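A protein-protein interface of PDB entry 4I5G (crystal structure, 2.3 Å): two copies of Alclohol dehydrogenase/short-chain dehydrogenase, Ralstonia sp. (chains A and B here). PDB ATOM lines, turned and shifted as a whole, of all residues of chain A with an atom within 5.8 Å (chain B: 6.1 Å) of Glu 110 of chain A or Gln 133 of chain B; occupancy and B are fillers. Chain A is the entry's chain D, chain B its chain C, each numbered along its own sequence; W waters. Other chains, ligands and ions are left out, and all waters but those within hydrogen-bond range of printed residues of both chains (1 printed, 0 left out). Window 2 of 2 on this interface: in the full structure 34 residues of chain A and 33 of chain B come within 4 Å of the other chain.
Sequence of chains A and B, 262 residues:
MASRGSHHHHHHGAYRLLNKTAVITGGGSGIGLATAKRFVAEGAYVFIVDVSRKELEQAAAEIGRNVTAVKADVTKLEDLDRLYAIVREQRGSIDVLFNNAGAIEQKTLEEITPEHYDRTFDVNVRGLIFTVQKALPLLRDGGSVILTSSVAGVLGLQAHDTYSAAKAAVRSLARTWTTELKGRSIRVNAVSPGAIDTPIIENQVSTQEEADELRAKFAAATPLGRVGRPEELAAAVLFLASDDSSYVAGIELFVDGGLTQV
The backbone carbonyl oxygen (O) of Ile 112 of chain A lies within hydrogen-bond range of the side-chain amide nitrogen (NE2) of Gln 133 of chain B (3.0 Å).
O of Leu 109 of chain A is in hydrogen-bond range of NE2 of Gln 133 of chain B (2.8 Å).
N of Leu 109 of chain A sits at hydrogen-bond distance from OE1 of Glu 180 of chain B (2.9 Å).
The side-chain carboxylate (OD1) of Asp 161 of chain A lies close to the side-chain carboxylate (OE2) of Glu 180 of chain B (2.4 Å).
The indole nitrogen of Trp 177 of chain B lies within hydrogen-bond range of the side-chain carboxylate of Asp 161 of chain A.
The side-chain amide nitrogen (NE2) of Gln 133 of chain B lies within hydrogen-bond range of the backbone carbonyl oxygen (O) of Glu 110 of chain A (3.3 Å).
OG1 of Thr 108 of chain A sits close to OE1 of Glu 111 of chain A.
N of Leu 109 of chain A is in hydrogen-bond range of OD2 of Asp 161 of chain A (3.2 Å).
Among the printed residues, merely in contact across the chains: Thr 108 of chain A with Glu 180 of chain B (3.5 Å), Leu 109 of chain A with Ile 129 of chain B (3.7 Å), Leu 109 of chain A with Val 132 of chain B (3.7 Å), Leu 109 of chain A with Trp 177 of chain B (3.6 Å), Ile 112 of chain A with Ile 129 of chain B (3.8 Å), Ile 112 of chain A with Phe 130 of chain B (3.7 Å) and Thr 113 of chain A with Phe 130 of chain B (3.9 Å).
Of chain B, only Gln 133 (3.3 Å) comes within 4 Å of Glu 110 of chain A.
Gln 133 of chain B touches three residues of chain A.
Printed residues of chain B within 4 Å of Thr 108 of chain A: Glu 180 (3.5 Å).
Of the printed residues of chain A, Trp 177 of chain B touches Leu 109 (3.6 Å) and Asp 161 (2.8 Å).
The nearest residue of chain B that does not touch Glu 110 of chain A is Leu 136 of chain B (4.1 Å).
The nearest residue of chain A that does not touch Gln 133 of chain B is Glu 111 of chain A (4.3 Å).
Hydrophobic or aromatic side chains of chain A that line the printed part of chain B: Leu 109 and Ile 112.
Printed residues of chain B that touch a printed residue of chain A: Ile 129, Phe 130, Val 132, Gln 133, Trp 177 and Glu 180.
Hydrophobic or aromatic side chains of chain B that line the printed part of chain A: Ile 129, Phe 130, Val 132 and Trp 177.
No position is printed for both chains.
Water W1 lies within hydrogen-bond range of OE1 of Glu 180 of chain B (2.8 Å), N of Glu 110 of chain A (3.4 Å) and N of Leu 109 of chain A (3.5 Å).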
ATOM      1  N   THR A 108       7.298  31.721  -0.199  1.00  0.00           N
ATOM      2  CA  THR A 108       7.550  30.512   0.570  1.00  0.00           C
ATOM      3  C   THR A 108       7.910  29.464  -0.488  1.00  0.00           C
ATOM      4  O   THR A 108       7.614  29.675  -1.698  1.00  0.00           O
ATOM      5  CB  THR A 108       6.251  30.090   1.238  1.00  0.00           C
ATOM      6  OG1 THR A 108       5.249  29.963   0.223  1.00  0.00           O
ATOM      7  CG2 THR A 108       5.780  31.204   2.253  1.00  0.00           C
ATOM      8  N   LEU A 109       8.544  28.369  -0.017  1.00  0.00           N
ATOM      9  CA  LEU A 109       8.887  27.223  -0.833  1.00  0.00           C
ATOM     10  C   LEU A 109       7.705  26.877  -1.737  1.00  0.00           C
ATOM     11  O   LEU A 109       7.842  26.623  -2.937  1.00  0.00           O
ATOM     12  CB  LEU A 109       9.184  26.013   0.052  1.00  0.00           C
ATOM     13  CG  LEU A 109       9.520  24.697  -0.644  1.00  0.00           C
ATOM     14  CD1 LEU A 109      10.573  24.975  -1.710  1.00  0.00           C
ATOM     15  CD2 LEU A 109      10.085  23.683   0.357  1.00  0.00           C
ATOM     16  N   GLU A 110       6.538  26.881  -1.127  1.00  0.00           N
ATOM     17  CA  GLU A 110       5.357  26.388  -1.750  1.00  0.00           C
ATOM     18  C   GLU A 110       4.939  27.240  -2.965  1.00  0.00           C
ATOM     19  O   GLU A 110       4.331  26.739  -3.904  1.00  0.00           O
ATOM     20  CB  GLU A 110       4.254  26.415  -0.702  1.00  0.00           C
ATOM     21  CG  GLU A 110       3.406  25.201  -0.798  1.00  0.00           C
ATOM     22  CD  GLU A 110       2.509  25.065   0.403  1.00  0.00           C
ATOM     23  OE1 GLU A 110       1.492  24.335   0.291  1.00  0.00           O
ATOM     24  OE2 GLU A 110       2.825  25.684   1.454  1.00  0.00           O
ATOM     25  N   GLU A 111       5.258  28.532  -2.885  1.00  0.00           N
ATOM     26  CA  GLU A 111       4.815  29.541  -3.822  1.00  0.00           C
ATOM     27  C   GLU A 111       5.924  29.785  -4.831  1.00  0.00           C
ATOM     28  O   GLU A 111       5.652  30.399  -5.841  1.00  0.00           O
ATOM     29  CB  GLU A 111       4.526  30.879  -3.114  1.00  0.00           C
ATOM     30  CG  GLU A 111       3.407  30.850  -2.052  1.00  0.00           C
ATOM     31  CD  GLU A 111       3.323  32.141  -1.182  1.00  0.00           C
ATOM     32  OE1 GLU A 111       4.352  32.852  -0.826  1.00  0.00           O
ATOM     33  OE2 GLU A 111       2.169  32.457  -0.824  1.00  0.00           O
ATOM     34  N   ILE A 112       7.143  29.301  -4.596  1.00  0.00           N
ATOM     35  CA  ILE A 112       8.208  29.515  -5.606  1.00  0.00           C
ATOM     36  C   ILE A 112       7.857  29.086  -7.050  1.00  0.00           C
ATOM     37  O   ILE A 112       7.468  27.971  -7.261  1.00  0.00           O
ATOM     38  CB  ILE A 112       9.503  28.834  -5.239  1.00  0.00           C
ATOM     39  CG1 ILE A 112      10.069  29.498  -3.975  1.00  0.00           C
ATOM     40  CG2 ILE A 112      10.499  28.954  -6.398  1.00  0.00           C
ATOM     41  CD1 ILE A 112      11.396  28.898  -3.432  1.00  0.00           C
ATOM     42  N   THR A 113       7.982  29.988  -8.007  1.00  0.00           N
ATOM     43  CA  THR A 113       7.870  29.670  -9.428  1.00  0.00           C
ATOM     44  C   THR A 113       9.249  29.786 -10.064  1.00  0.00           C
ATOM     45  O   THR A 113      10.132  30.410  -9.496  1.00  0.00           O
ATOM     46  CB  THR A 113       7.031  30.732 -10.209  1.00  0.00           C
ATOM     47  OG1 THR A 113       7.715  32.021 -10.165  1.00  0.00           O
ATOM     48  CG2 THR A 113       5.552  30.758  -9.713  1.00  0.00           C
ATOM     49  N   ASP A 161      13.152  32.177   1.170  1.00  0.00           N
ATOM     50  CA  ASP A 161      13.911  31.058   0.597  1.00  0.00           C
ATOM     51  C   ASP A 161      15.035  31.459  -0.382  1.00  0.00           C
ATOM     52  O   ASP A 161      16.223  31.144  -0.142  1.00  0.00           O
ATOM     53  CB  ASP A 161      13.043  29.994  -0.061  1.00  0.00           C
ATOM     54  CG  ASP A 161      11.876  29.563   0.791  1.00  0.00           C
ATOM     55  OD1 ASP A 161      11.196  30.491   1.368  1.00  0.00           O
ATOM     56  OD2 ASP A 161      11.655  28.305   0.844  1.00  0.00           O
ATOM     57  N   TYR B  84       6.938  11.597  -8.168  1.00  0.00           N
ATOM     58  CA  TYR B  84       6.138  11.548  -6.964  1.00  0.00           C
ATOM     59  C   TYR B  84       4.834  10.794  -7.197  1.00  0.00           C
ATOM     60  O   TYR B  84       4.273  10.196  -6.278  1.00  0.00           O
ATOM     61  CB  TYR B  84       5.951  12.941  -6.378  1.00  0.00           C
ATOM     62  CG  TYR B  84       7.269  13.480  -5.859  1.00  0.00           C
ATOM     63  CD1 TYR B  84       7.949  12.829  -4.846  1.00  0.00           C
ATOM     64  CD2 TYR B  84       7.818  14.673  -6.376  1.00  0.00           C
ATOM     65  CE1 TYR B  84       9.163  13.334  -4.371  1.00  0.00           C
ATOM     66  CE2 TYR B  84       9.027  15.193  -5.917  1.00  0.00           C
ATOM     67  CZ  TYR B  84       9.728  14.529  -4.926  1.00  0.00           C
ATOM     68  OH  TYR B  84      10.994  15.056  -4.467  1.00  0.00           O
ATOM     69  N   LEU B 128      16.720  21.323  -6.649  1.00  0.00           N
ATOM     70  CA  LEU B 128      16.577  20.950  -5.223  1.00  0.00           C
ATOM     71  C   LEU B 128      15.364  21.625  -4.703  1.00  0.00           C
ATOM     72  O   LEU B 128      14.456  20.969  -4.211  1.00  0.00           O
ATOM     73  CB  LEU B 128      17.795  21.380  -4.437  1.00  0.00           C
ATOM     74  CG  LEU B 128      17.699  21.186  -2.928  1.00  0.00           C
ATOM     75  CD1 LEU B 128      17.694  19.679  -2.632  1.00  0.00           C
ATOM     76  CD2 LEU B 128      18.790  21.955  -2.174  1.00  0.00           C
ATOM     77  N   ILE B 129      15.257  22.925  -4.935  1.00  0.00           N
ATOM     78  CA  ILE B 129      14.018  23.658  -4.579  1.00  0.00           C
ATOM     79  C   ILE B 129      12.799  22.953  -5.054  1.00  0.00           C
ATOM     80  O   ILE B 129      11.933  22.710  -4.259  1.00  0.00           O
ATOM     81  CB  ILE B 129      14.048  25.098  -5.123  1.00  0.00           C
ATOM     82  CG1 ILE B 129      15.173  25.881  -4.368  1.00  0.00           C
ATOM     83  CG2 ILE B 129      12.642  25.761  -5.139  1.00  0.00           C
ATOM     84  CD1 ILE B 129      15.440  27.295  -4.862  1.00  0.00           C
ATOM     85  N   PHE B 130      12.718  22.590  -6.320  1.00  0.00           N
ATOM     86  CA  PHE B 130      11.466  22.024  -6.886  1.00  0.00           C
ATOM     87  C   PHE B 130      11.293  20.596  -6.484  1.00  0.00           C
ATOM     88  O   PHE B 130      10.176  20.125  -6.293  1.00  0.00           O
ATOM     89  CB  PHE B 130      11.408  22.184  -8.385  1.00  0.00           C
ATOM     90  CG  PHE B 130      11.186  23.613  -8.778  1.00  0.00           C
ATOM     91  CD1 PHE B 130       9.955  24.223  -8.551  1.00  0.00           C
ATOM     92  CD2 PHE B 130      12.215  24.374  -9.315  1.00  0.00           C
ATOM     93  CE1 PHE B 130       9.741  25.553  -8.886  1.00  0.00           C
ATOM     94  CE2 PHE B 130      12.018  25.719  -9.652  1.00  0.00           C
ATOM     95  CZ  PHE B 130      10.799  26.320  -9.409  1.00  0.00           C
ATOM     96  N   THR B 131      12.431  19.946  -6.257  1.00  0.00           N
ATOM     97  CA  THR B 131      12.421  18.575  -5.652  1.00  0.00           C
ATOM     98  C   THR B 131      11.703  18.517  -4.326  1.00  0.00           C
ATOM     99  O   THR B 131      10.727  17.744  -4.180  1.00  0.00           O
ATOM    100  CB  THR B 131      13.804  17.955  -5.612  1.00  0.00           C
ATOM    101  OG1 THR B 131      14.362  18.025  -6.944  1.00  0.00           O
ATOM    102  CG2 THR B 131      13.701  16.524  -5.186  1.00  0.00           C
ATOM    103  N   VAL B 132      12.112  19.390  -3.410  1.00  0.00           N
ATOM    104  CA  VAL B 132      11.583  19.385  -2.025  1.00  0.00           C
ATOM    105  C   VAL B 132      10.174  19.994  -2.124  1.00  0.00           C
ATOM    106  O   VAL B 132       9.224  19.512  -1.404  1.00  0.00           O
ATOM    107  CB  VAL B 132      12.528  20.182  -1.029  1.00  0.00           C
ATOM    108  CG1 VAL B 132      11.881  20.435   0.312  1.00  0.00           C
ATOM    109  CG2 VAL B 132      13.892  19.478  -0.882  1.00  0.00           C
ATOM    110  N   GLN B 133      10.023  20.998  -3.031  1.00  0.00           N
ATOM    111  CA  GLN B 133       8.681  21.633  -3.271  1.00  0.00           C
ATOM    112  C   GLN B 133       7.622  20.580  -3.587  1.00  0.00           C
ATOM    113  O   GLN B 133       6.550  20.601  -3.042  1.00  0.00           O
ATOM    114  CB  GLN B 133       8.653  22.676  -4.417  1.00  0.00           C
ATOM    115  CG  GLN B 133       7.284  23.387  -4.532  1.00  0.00           C
ATOM    116  CD  GLN B 133       7.198  24.341  -5.738  1.00  0.00           C
ATOM    117  OE1 GLN B 133       7.201  23.924  -6.925  1.00  0.00           O
ATOM    118  NE2 GLN B 133       7.077  25.631  -5.448  1.00  0.00           N
ATOM    119  N   LYS B 134       7.927  19.661  -4.498  1.00  0.00           N
ATOM    120  CA  LYS B 134       6.851  18.777  -5.004  1.00  0.00           C
ATOM    121  C   LYS B 134       6.766  17.575  -4.103  1.00  0.00           C
ATOM    122  O   LYS B 134       5.772  16.837  -4.156  1.00  0.00           O
ATOM    123  CB  LYS B 134       7.087  18.387  -6.488  1.00  0.00           C
ATOM    124  CG  LYS B 134       6.972  19.567  -7.423  1.00  0.00           C
ATOM    125  CD  LYS B 134       7.371  19.210  -8.831  1.00  0.00           C
ATOM    126  CE  LYS B 134       6.983  20.323  -9.833  1.00  0.00           C
ATOM    127  NZ  LYS B 134       5.528  20.250 -10.118  1.00  0.00           N
ATOM    128  N   ALA B 135       7.781  17.419  -3.249  1.00  0.00           N
ATOM    129  CA  ALA B 135       7.711  16.447  -2.139  1.00  0.00           C
ATOM    130  C   ALA B 135       6.749  16.819  -1.003  1.00  0.00           C
ATOM    131  O   ALA B 135       6.248  15.963  -0.374  1.00  0.00           O
ATOM    132  CB  ALA B 135       9.105  16.126  -1.601  1.00  0.00           C
ATOM    133  N   LEU B 136       6.463  18.089  -0.754  1.00  0.00           N
ATOM    134  CA  LEU B 136       5.630  18.495   0.375  1.00  0.00           C
ATOM    135  C   LEU B 136       4.312  17.757   0.569  1.00  0.00           C
ATOM    136  O   LEU B 136       4.048  17.301   1.706  1.00  0.00           O
ATOM    137  CB  LEU B 136       5.363  19.998   0.406  1.00  0.00           C
ATOM    138  CG  LEU B 136       6.572  20.898   0.503  1.00  0.00           C
ATOM    139  CD1 LEU B 136       6.211  22.397   0.309  1.00  0.00           C
ATOM    140  CD2 LEU B 136       7.389  20.617   1.763  1.00  0.00           C
ATOM    141  N   PRO B 137       3.483  17.657  -0.489  1.00  0.00           N
ATOM    142  CA  PRO B 137       2.236  16.916  -0.152  1.00  0.00           C
ATOM    143  C   PRO B 137       2.464  15.473   0.283  1.00  0.00           C
ATOM    144  O   PRO B 137       1.591  14.925   0.882  1.00  0.00           O
ATOM    145  CB  PRO B 137       1.347  16.985  -1.446  1.00  0.00           C
ATOM    146  CG  PRO B 137       2.006  18.093  -2.328  1.00  0.00           C
ATOM    147  CD  PRO B 137       3.466  18.259  -1.867  1.00  0.00           C
ATOM    148  N   TRP B 177      13.882  26.272   5.448  1.00  0.00           N
ATOM    149  CA  TRP B 177      12.819  25.263   5.414  1.00  0.00           C
ATOM    150  C   TRP B 177      12.603  24.692   6.773  1.00  0.00           C
ATOM    151  O   TRP B 177      11.535  24.171   7.047  1.00  0.00           O
ATOM    152  CB  TRP B 177      13.120  24.145   4.387  1.00  0.00           C
ATOM    153  CG  TRP B 177      13.238  24.604   2.964  1.00  0.00           C
ATOM    154  CD1 TRP B 177      12.623  25.708   2.382  1.00  0.00           C
ATOM    155  CD2 TRP B 177      13.989  23.983   1.874  1.00  0.00           C
ATOM    156  NE1 TRP B 177      12.912  25.809   1.052  1.00  0.00           N
ATOM    157  CE2 TRP B 177      13.726  24.814   0.670  1.00  0.00           C
ATOM    158  CE3 TRP B 177      14.808  22.855   1.754  1.00  0.00           C
ATOM    159  CZ2 TRP B 177      14.286  24.512  -0.576  1.00  0.00           C
ATOM    160  CZ3 TRP B 177      15.370  22.570   0.502  1.00  0.00           C
ATOM    161  CH2 TRP B 177      15.105  23.372  -0.641  1.00  0.00           C
ATOM    162  N   GLU B 180      10.053  27.155   7.787  1.00  0.00           N
ATOM    163  CA  GLU B 180       8.808  27.105   7.059  1.00  0.00           C
ATOM    164  C   GLU B 180       7.982  25.819   7.338  1.00  0.00           C
ATOM    165  O   GLU B 180       6.820  25.799   7.126  1.00  0.00           O
ATOM    166  CB  GLU B 180       9.077  27.309   5.556  1.00  0.00           C
ATOM    167  CG  GLU B 180       9.418  28.767   5.184  1.00  0.00           C
ATOM    168  CD  GLU B 180       9.352  29.066   3.662  1.00  0.00           C
ATOM    169  OE1 GLU B 180       8.855  28.200   2.863  1.00  0.00           O
ATOM    170  OE2 GLU B 180       9.794  30.174   3.250  1.00  0.00           O
HETATM  171  O   HOH W   1       6.688  26.517   2.246  1.00  0.00           O
